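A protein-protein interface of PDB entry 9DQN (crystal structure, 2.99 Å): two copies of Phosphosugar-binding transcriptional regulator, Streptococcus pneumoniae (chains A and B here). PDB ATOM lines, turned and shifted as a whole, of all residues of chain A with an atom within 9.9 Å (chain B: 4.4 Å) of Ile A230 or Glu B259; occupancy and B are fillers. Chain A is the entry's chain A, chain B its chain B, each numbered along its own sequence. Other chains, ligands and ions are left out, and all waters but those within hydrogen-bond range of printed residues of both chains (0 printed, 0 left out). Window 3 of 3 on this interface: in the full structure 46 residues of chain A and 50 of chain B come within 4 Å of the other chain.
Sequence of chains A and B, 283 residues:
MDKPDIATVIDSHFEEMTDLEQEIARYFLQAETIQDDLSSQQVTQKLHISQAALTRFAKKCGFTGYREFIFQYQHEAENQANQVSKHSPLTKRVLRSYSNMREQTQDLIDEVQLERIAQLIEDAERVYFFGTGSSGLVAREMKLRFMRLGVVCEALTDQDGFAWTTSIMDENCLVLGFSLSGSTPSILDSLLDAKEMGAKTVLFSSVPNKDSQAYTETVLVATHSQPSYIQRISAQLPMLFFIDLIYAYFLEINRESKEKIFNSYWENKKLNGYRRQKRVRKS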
ATOM      1  N   ARG A  93     -16.842 -16.809  17.192  1.00  0.00           N
ATOM      2  CA  ARG A  93     -17.827 -15.735  17.232  1.00  0.00           C
ATOM      3  C   ARG A  93     -17.164 -14.364  17.139  1.00  0.00           C
ATOM      4  O   ARG A  93     -17.674 -13.470  16.453  1.00  0.00           O
ATOM      5  CB  ARG A  93     -18.666 -15.854  18.505  1.00  0.00           C
ATOM      6  CG  ARG A  93     -19.795 -14.847  18.611  1.00  0.00           C
ATOM      7  CD  ARG A  93     -19.477 -13.775  19.637  1.00  0.00           C
ATOM      8  NE  ARG A  93     -19.436 -14.313  20.990  1.00  0.00           N
ATOM      9  CZ  ARG A  93     -19.202 -13.590  22.077  1.00  0.00           C
ATOM     10  NH1 ARG A  93     -18.968 -12.290  22.003  1.00  0.00           N
ATOM     11  NH2 ARG A  93     -19.204 -14.184  23.266  1.00  0.00           N
ATOM     12  N   VAL A  94     -16.032 -14.178  17.822  1.00  0.00           N
ATOM     13  CA  VAL A  94     -15.346 -12.888  17.795  1.00  0.00           C
ATOM     14  C   VAL A  94     -14.787 -12.604  16.405  1.00  0.00           C
ATOM     15  O   VAL A  94     -14.905 -11.485  15.892  1.00  0.00           O
ATOM     16  CB  VAL A  94     -14.246 -12.846  18.871  1.00  0.00           C
ATOM     17  CG1 VAL A  94     -13.457 -11.547  18.779  1.00  0.00           C
ATOM     18  CG2 VAL A  94     -14.856 -13.001  20.254  1.00  0.00           C
ATOM     19  N   HIS A 224     -22.945  -3.206  15.252  1.00  0.00           N
ATOM     20  CA  HIS A 224     -22.322  -4.373  15.857  1.00  0.00           C
ATOM     21  C   HIS A 224     -23.084  -5.648  15.506  1.00  0.00           C
ATOM     22  O   HIS A 224     -24.317  -5.677  15.507  1.00  0.00           O
ATOM     23  CB  HIS A 224     -22.227  -4.198  17.371  1.00  0.00           C
ATOM     24  CG  HIS A 224     -21.154  -3.243  17.800  1.00  0.00           C
ATOM     25  ND1 HIS A 224     -19.827  -3.608  17.888  1.00  0.00           N
ATOM     26  CD2 HIS A 224     -21.208  -1.937  18.153  1.00  0.00           C
ATOM     27  CE1 HIS A 224     -19.112  -2.569  18.281  1.00  0.00           C
ATOM     28  NE2 HIS A 224     -19.925  -1.544  18.450  1.00  0.00           N
ATOM     29  N   GLN A 226     -23.163  -8.548  17.143  1.00  0.00           N
ATOM     30  CA  GLN A 226     -23.828  -9.151  18.288  1.00  0.00           C
ATOM     31  C   GLN A 226     -25.097  -8.377  18.639  1.00  0.00           C
ATOM     32  O   GLN A 226     -25.087  -7.142  18.668  1.00  0.00           O
ATOM     33  CB  GLN A 226     -22.890  -9.189  19.492  1.00  0.00           C
ATOM     34  CG  GLN A 226     -21.865 -10.305  19.431  1.00  0.00           C
ATOM     35  CD  GLN A 226     -22.507 -11.675  19.487  1.00  0.00           C
ATOM     36  OE1 GLN A 226     -23.203 -12.009  20.445  1.00  0.00           O
ATOM     37  NE2 GLN A 226     -22.283 -12.477  18.451  1.00  0.00           N
ATOM     38  N   PRO A 227     -26.206  -9.071  18.905  1.00  0.00           N
ATOM     39  CA  PRO A 227     -27.433  -8.375  19.314  1.00  0.00           C
ATOM     40  C   PRO A 227     -27.390  -7.941  20.771  1.00  0.00           C
ATOM     41  O   PRO A 227     -27.811  -6.831  21.109  1.00  0.00           O
ATOM     42  CB  PRO A 227     -28.524  -9.422  19.066  1.00  0.00           C
ATOM     43  CG  PRO A 227     -27.823 -10.734  19.229  1.00  0.00           C
ATOM     44  CD  PRO A 227     -26.408 -10.524  18.755  1.00  0.00           C
ATOM     45  N   SER A 228     -26.883  -8.813  21.639  1.00  0.00           N
ATOM     46  CA  SER A 228     -26.772  -8.505  23.059  1.00  0.00           C
ATOM     47  C   SER A 228     -25.567  -7.606  23.302  1.00  0.00           C
ATOM     48  O   SER A 228     -24.474  -7.871  22.792  1.00  0.00           O
ATOM     49  CB  SER A 228     -26.649  -9.794  23.871  1.00  0.00           C
ATOM     50  OG  SER A 228     -26.648  -9.524  25.260  1.00  0.00           O
ATOM     51  N   TYR A 229     -25.767  -6.550  24.098  1.00  0.00           N
ATOM     52  CA  TYR A 229     -24.732  -5.533  24.271  1.00  0.00           C
ATOM     53  C   TYR A 229     -23.475  -6.112  24.913  1.00  0.00           C
ATOM     54  O   TYR A 229     -22.354  -5.754  24.530  1.00  0.00           O
ATOM     55  CB  TYR A 229     -25.271  -4.372  25.108  1.00  0.00           C
ATOM     56  CG  TYR A 229     -24.577  -3.047  24.859  1.00  0.00           C
ATOM     57  CD1 TYR A 229     -23.224  -2.884  25.134  1.00  0.00           C
ATOM     58  CD2 TYR A 229     -25.278  -1.956  24.361  1.00  0.00           C
ATOM     59  CE1 TYR A 229     -22.587  -1.680  24.907  1.00  0.00           C
ATOM     60  CE2 TYR A 229     -24.649  -0.743  24.134  1.00  0.00           C
ATOM     61  CZ  TYR A 229     -23.302  -0.613  24.409  1.00  0.00           C
ATOM     62  OH  TYR A 229     -22.668   0.589  24.188  1.00  0.00           O
ATOM     63  N   ILE A 230     -23.639  -7.005  25.893  1.00  0.00           N
ATOM     64  CA  ILE A 230     -22.500  -7.494  26.666  1.00  0.00           C
ATOM     65  C   ILE A 230     -21.503  -8.235  25.783  1.00  0.00           C
ATOM     66  O   ILE A 230     -20.305  -8.277  26.089  1.00  0.00           O
ATOM     67  CB  ILE A 230     -22.985  -8.385  27.828  1.00  0.00           C
ATOM     68  CG1 ILE A 230     -24.255  -7.813  28.461  1.00  0.00           C
ATOM     69  CG2 ILE A 230     -21.905  -8.510  28.891  1.00  0.00           C
ATOM     70  CD1 ILE A 230     -25.531  -8.519  28.054  1.00  0.00           C
ATOM     71  N   GLN A 231     -21.969  -8.829  24.685  1.00  0.00           N
ATOM     72  CA  GLN A 231     -21.127  -9.668  23.843  1.00  0.00           C
ATOM     73  C   GLN A 231     -20.554  -8.942  22.632  1.00  0.00           C
ATOM     74  O   GLN A 231     -19.777  -9.544  21.883  1.00  0.00           O
ATOM     75  CB  GLN A 231     -21.912 -10.898  23.379  1.00  0.00           C
ATOM     76  CG  GLN A 231     -22.381 -11.796  24.512  1.00  0.00           C
ATOM     77  CD  GLN A 231     -22.901 -13.132  24.019  1.00  0.00           C
ATOM     78  OE1 GLN A 231     -23.091 -14.063  24.801  1.00  0.00           O
ATOM     79  NE2 GLN A 231     -23.131 -13.233  22.716  1.00  0.00           N
ATOM     80  N   ARG A 232     -20.907  -7.678  22.417  1.00  0.00           N
ATOM     81  CA  ARG A 232     -20.430  -6.967  21.239  1.00  0.00           C
ATOM     82  C   ARG A 232     -18.944  -6.645  21.366  1.00  0.00           C
ATOM     83  O   ARG A 232     -18.423  -6.414  22.461  1.00  0.00           O
ATOM     84  CB  ARG A 232     -21.235  -5.684  21.024  1.00  0.00           C
ATOM     85  CG  ARG A 232     -22.708  -5.851  21.344  1.00  0.00           C
ATOM     86  CD  ARG A 232     -23.617  -4.923  20.558  1.00  0.00           C
ATOM     87  NE  ARG A 232     -23.339  -3.512  20.795  1.00  0.00           N
ATOM     88  CZ  ARG A 232     -24.203  -2.534  20.563  1.00  0.00           C
ATOM     89  NH1 ARG A 232     -25.425  -2.781  20.120  1.00  0.00           N
ATOM     90  NH2 ARG A 232     -23.835  -1.276  20.789  1.00  0.00           N
ATOM     91  N   ILE A 233     -18.261  -6.628  20.221  1.00  0.00           N
ATOM     92  CA  ILE A 233     -16.829  -6.344  20.164  1.00  0.00           C
ATOM     93  C   ILE A 233     -16.585  -4.869  20.453  1.00  0.00           C
ATOM     94  O   ILE A 233     -17.508  -4.137  20.828  1.00  0.00           O
ATOM     95  CB  ILE A 233     -16.233  -6.748  18.804  1.00  0.00           C
ATOM     96  CG1 ILE A 233     -17.227  -6.463  17.676  1.00  0.00           C
ATOM     97  CG2 ILE A 233     -15.820  -8.214  18.812  1.00  0.00           C
ATOM     98  CD1 ILE A 233     -16.653  -6.667  16.292  1.00  0.00           C
ATOM     99  N   SER A 234     -15.337  -4.429  20.294  1.00  0.00           N
ATOM    100  CA  SER A 234     -14.963  -3.060  20.631  1.00  0.00           C
ATOM    101  C   SER A 234     -15.817  -2.054  19.867  1.00  0.00           C
ATOM    102  O   SER A 234     -16.022  -2.184  18.657  1.00  0.00           O
ATOM    103  CB  SER A 234     -13.483  -2.832  20.324  1.00  0.00           C
ATOM    104  OG  SER A 234     -13.133  -1.468  20.486  1.00  0.00           O
ATOM    105  N   LEU B 149     -17.647  -5.114  34.073  1.00  0.00           N
ATOM    106  CA  LEU B 149     -17.861  -6.480  34.531  1.00  0.00           C
ATOM    107  C   LEU B 149     -17.432  -6.700  35.977  1.00  0.00           C
ATOM    108  O   LEU B 149     -17.492  -7.836  36.458  1.00  0.00           O
ATOM    109  CB  LEU B 149     -17.122  -7.468  33.621  1.00  0.00           C
ATOM    110  CG  LEU B 149     -17.587  -7.562  32.165  1.00  0.00           C
ATOM    111  CD1 LEU B 149     -16.888  -8.712  31.454  1.00  0.00           C
ATOM    112  CD2 LEU B 149     -19.098  -7.720  32.085  1.00  0.00           C
ATOM    113  N   TYR B 247     -11.666 -10.742  26.304  1.00  0.00           N
ATOM    114  CA  TYR B 247     -12.915 -10.294  26.911  1.00  0.00           C
ATOM    115  C   TYR B 247     -13.994 -11.365  26.811  1.00  0.00           C
ATOM    116  O   TYR B 247     -14.714 -11.621  27.782  1.00  0.00           O
ATOM    117  CB  TYR B 247     -13.383  -8.998  26.247  1.00  0.00           C
ATOM    118  CG  TYR B 247     -14.732  -8.509  26.724  1.00  0.00           C
ATOM    119  CD1 TYR B 247     -15.880  -8.727  25.971  1.00  0.00           C
ATOM    120  CD2 TYR B 247     -14.858  -7.830  27.926  1.00  0.00           C
ATOM    121  CE1 TYR B 247     -17.114  -8.281  26.404  1.00  0.00           C
ATOM    122  CE2 TYR B 247     -16.086  -7.380  28.366  1.00  0.00           C
ATOM    123  CZ  TYR B 247     -17.211  -7.607  27.604  1.00  0.00           C
ATOM    124  OH  TYR B 247     -18.431  -7.155  28.051  1.00  0.00           O
ATOM    125  N   LEU B 251     -15.502 -13.236  30.010  1.00  0.00           N
ATOM    126  CA  LEU B 251     -16.915 -13.061  30.332  1.00  0.00           C
ATOM    127  C   LEU B 251     -17.577 -14.377  30.719  1.00  0.00           C
ATOM    128  O   LEU B 251     -18.481 -14.386  31.562  1.00  0.00           O
ATOM    129  CB  LEU B 251     -17.645 -12.423  29.149  1.00  0.00           C
ATOM    130  CG  LEU B 251     -19.136 -12.110  29.285  1.00  0.00           C
ATOM    131  CD1 LEU B 251     -19.442 -11.450  30.622  1.00  0.00           C
ATOM    132  CD2 LEU B 251     -19.573 -11.214  28.139  1.00  0.00           C
ATOM    133  N   ARG B 255     -20.200 -16.211  34.372  1.00  0.00           N
ATOM    134  CA  ARG B 255     -20.980 -15.355  33.483  1.00  0.00           C
ATOM    135  C   ARG B 255     -22.226 -14.821  34.177  1.00  0.00           C
ATOM    136  O   ARG B 255     -22.598 -13.655  33.991  1.00  0.00           O
ATOM    137  CB  ARG B 255     -21.365 -16.127  32.219  1.00  0.00           C
ATOM    138  CG  ARG B 255     -22.488 -15.484  31.415  1.00  0.00           C
ATOM    139  CD  ARG B 255     -21.966 -14.724  30.207  1.00  0.00           C
ATOM    140  NE  ARG B 255     -23.011 -13.917  29.587  1.00  0.00           N
ATOM    141  CZ  ARG B 255     -23.088 -13.658  28.288  1.00  0.00           C
ATOM    142  NH1 ARG B 255     -22.216 -14.163  27.430  1.00  0.00           N
ATOM    143  NH2 ARG B 255     -24.070 -12.882  27.839  1.00  0.00           N
ATOM    144  N   GLU B 256     -22.885 -15.660  34.978  1.00  0.00           N
ATOM    145  CA  GLU B 256     -24.119 -15.248  35.638  1.00  0.00           C
ATOM    146  C   GLU B 256     -23.876 -14.075  36.579  1.00  0.00           C
ATOM    147  O   GLU B 256     -24.628 -13.094  36.575  1.00  0.00           O
ATOM    148  CB  GLU B 256     -24.731 -16.433  36.392  1.00  0.00           C
ATOM    149  CG  GLU B 256     -25.342 -17.507  35.497  1.00  0.00           C
ATOM    150  CD  GLU B 256     -24.308 -18.258  34.675  1.00  0.00           C
ATOM    151  OE1 GLU B 256     -23.303 -18.720  35.256  1.00  0.00           O
ATOM    152  OE2 GLU B 256     -24.496 -18.375  33.445  1.00  0.00           O
ATOM    153  N   SER B 257     -22.815 -14.149  37.386  1.00  0.00           N
ATOM    154  CA  SER B 257     -22.524 -13.064  38.318  1.00  0.00           C
ATOM    155  C   SER B 257     -22.021 -11.823  37.589  1.00  0.00           C
ATOM    156  O   SER B 257     -22.339 -10.694  37.983  1.00  0.00           O
ATOM    157  CB  SER B 257     -21.503 -13.525  39.358  1.00  0.00           C
ATOM    158  OG  SER B 257     -20.280 -13.890  38.747  1.00  0.00           O
ATOM    159  N   LYS B 258     -21.234 -12.008  36.526  1.00  0.00           N
ATOM    160  CA  LYS B 258     -20.657 -10.864  35.825  1.00  0.00           C
ATOM    161  C   LYS B 258     -21.714 -10.072  35.069  1.00  0.00           C
ATOM    162  O   LYS B 258     -21.621  -8.843  34.970  1.00  0.00           O
ATOM    163  CB  LYS B 258     -19.556 -11.328  34.876  1.00  0.00           C
ATOM    164  CG  LYS B 258     -18.186 -11.296  35.508  1.00  0.00           C
ATOM    165  CD  LYS B 258     -17.200 -12.134  34.733  1.00  0.00           C
ATOM    166  CE  LYS B 258     -15.972 -12.390  35.576  1.00  0.00           C
ATOM    167  NZ  LYS B 258     -15.091 -13.431  34.978  1.00  0.00           N
ATOM    168  N   GLU B 259     -22.717 -10.755  34.513  1.00  0.00           N
ATOM    169  CA  GLU B 259     -23.784 -10.043  33.818  1.00  0.00           C
ATOM    170  C   GLU B 259     -24.565  -9.157  34.780  1.00  0.00           C
ATOM    171  O   GLU B 259     -24.927  -8.026  34.439  1.00  0.00           O
ATOM    172  CB  GLU B 259     -24.709 -11.037  33.115  1.00  0.00           C
ATOM    173  CG  GLU B 259     -25.542 -10.425  32.002  1.00  0.00           C
ATOM    174  CD  GLU B 259     -25.982 -11.449  30.975  1.00  0.00           C
ATOM    175  OE1 GLU B 259     -25.656 -12.642  31.148  1.00  0.00           O
ATOM    176  OE2 GLU B 259     -26.649 -11.062  29.991  1.00  0.00           O
ATOM    177  N   LYS B 260     -24.815  -9.648  35.998  1.00  0.00           N
ATOM    178  CA  LYS B 260     -25.506  -8.838  36.996  1.00  0.00           C
ATOM    179  C   LYS B 260     -24.717  -7.577  37.327  1.00  0.00           C
ATOM    180  O   LYS B 260     -25.303  -6.515  37.568  1.00  0.00           O
ATOM    181  CB  LYS B 260     -25.762  -9.667  38.255  1.00  0.00           C
ATOM    182  CG  LYS B 260     -27.235  -9.954  38.520  1.00  0.00           C
ATOM    183  CD  LYS B 260     -27.952 -10.426  37.260  1.00  0.00           C
ATOM    184  CE  LYS B 260     -27.483 -11.806  36.826  1.00  0.00           C
ATOM    185  NZ  LYS B 260     -27.996 -12.168  35.475  1.00  0.00           N
ATOM    186  N   ILE B 261     -23.385  -7.674  37.348  1.00  0.00           N
ATOM    187  CA  ILE B 261     -22.561  -6.484  37.532  1.00  0.00           C
ATOM    188  C   ILE B 261     -22.703  -5.546  36.338  1.00  0.00           C
ATOM    189  O   ILE B 261     -22.781  -4.322  36.498  1.00  0.00           O
ATOM    190  CB  ILE B 261     -21.093  -6.878  37.773  1.00  0.00           C
ATOM    191  CG1 ILE B 261     -20.981  -7.832  38.963  1.00  0.00           C
ATOM    192  CG2 ILE B 261     -20.242  -5.640  38.007  1.00  0.00           C
ATOM    193  CD1 ILE B 261     -21.482  -7.244  40.264  1.00  0.00           C
ATOM    194  N   PHE B 262     -22.728  -6.103  35.125  1.00  0.00           N
ATOM    195  CA  PHE B 262     -22.874  -5.278  33.929  1.00  0.00           C
ATOM    196  C   PHE B 262     -24.219  -4.563  33.912  1.00  0.00           C
ATOM    197  O   PHE B 262     -24.292  -3.356  33.654  1.00  0.00           O
ATOM    198  CB  PHE B 262     -22.709  -6.142  32.677  1.00  0.00           C
ATOM    199  CG  PHE B 262     -22.922  -5.395  31.388  1.00  0.00           C
ATOM    200  CD1 PHE B 262     -24.188  -5.283  30.834  1.00  0.00           C
ATOM    201  CD2 PHE B 262     -21.855  -4.810  30.729  1.00  0.00           C
ATOM    202  CE1 PHE B 262     -24.386  -4.594  29.652  1.00  0.00           C
ATOM    203  CE2 PHE B 262     -22.046  -4.123  29.544  1.00  0.00           C
ATOM    204  CZ  PHE B 262     -23.313  -4.016  29.005  1.00  0.00           C
ATOM    205  N   ASN B 263     -25.302  -5.300  34.174  1.00  0.00           N
ATOM    206  CA  ASN B 263     -26.635  -4.714  34.085  1.00  0.00           C
ATOM    207  C   ASN B 263     -26.842  -3.636  35.141  1.00  0.00           C
ATOM    208  O   ASN B 263     -27.512  -2.629  34.882  1.00  0.00           O
ATOM    209  CB  ASN B 263     -27.699  -5.806  34.200  1.00  0.00           C
ATOM    210  CG  ASN B 263     -27.741  -6.712  32.980  1.00  0.00           C
ATOM    211  OD1 ASN B 263     -27.219  -7.826  32.999  1.00  0.00           O
ATOM    212  ND2 ASN B 263     -28.363  -6.233  31.911  1.00  0.00           N
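OH of Tyr B247 lies within hydrogen-bond range of O of Ile A230, at 2.9 Å.
NH1 of Arg B255 sits at hydrogen-bond distance from OE1 of Gln A231, 2.8 Å away.
The backbone carbonyl oxygen (O) of Glu B259 sits close to the side-chain amide oxygen (OD1) of Asn B263.
The side-chain amide oxygen of Gln A226 is in hydrogen-bond range of the side-chain amide nitrogen of Gln A231, 2.6 Å away.
OE1 of Glu B259 lies within salt-bridge range of NE of Arg B255 (3.3 Å).
The guanidinium group (NH1) of Arg A93 lies within hydrogen-bond range of the backbone carbonyl oxygen (O) of Gln A231 (2.9 Å).
CG2 of Ile A230 touches CD2 of Leu B251, 3.6 Å away.
Glu B259 touches Ile A230.
Ile A230 touches Phe B262.
His A224 touches none of the printed residues of chain B.
Of chain B, only Tyr B247 (2.9 Å), Leu B251 (3.6 Å), Glu B259 (3.4 Å) and Phe B262 (3.4 Å) come within 4 Å of Ile A230.
Printed residues of chain B within 4 Å of Gln A231: Arg B255 (2.8 Å).
Of the printed residues of chain A, Tyr B247 touches Ile A230 (2.9 Å).
Printed residues of chain A within 4 Å of Leu B251: Ile A230 (3.6 Å).
Printed residues of chain A within 4 Å of Arg B255: Gln A231.
No residue of chain A comes within 4 Å of Ser B257.
Of chain A, only Ile A230 (3.4 Å) comes within 4 Å of Glu B259.
Of the printed residues of chain A, Phe B262 touches Ile A230 (3.4 Å).
Of the 12 printed residues of chain B, 5 touch a printed residue of chain A.
Of the 12 printed residues of chain A, 2 touch a printed residue of chain B.
Printed residues of chain A that touch a printed residue of chain B: Ile A230 and Gln A231.
Hydrophobic or aromatic side chains of chain A within 4 Å of the printed part of chain B: Ile A230.
Among the printed residues, 5 pairs touch across the chains.
No position is printed for both chains.
Of the 5 pairs that touch across the chains among the printed residues, none has its exchanged pair printed and touching as well.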
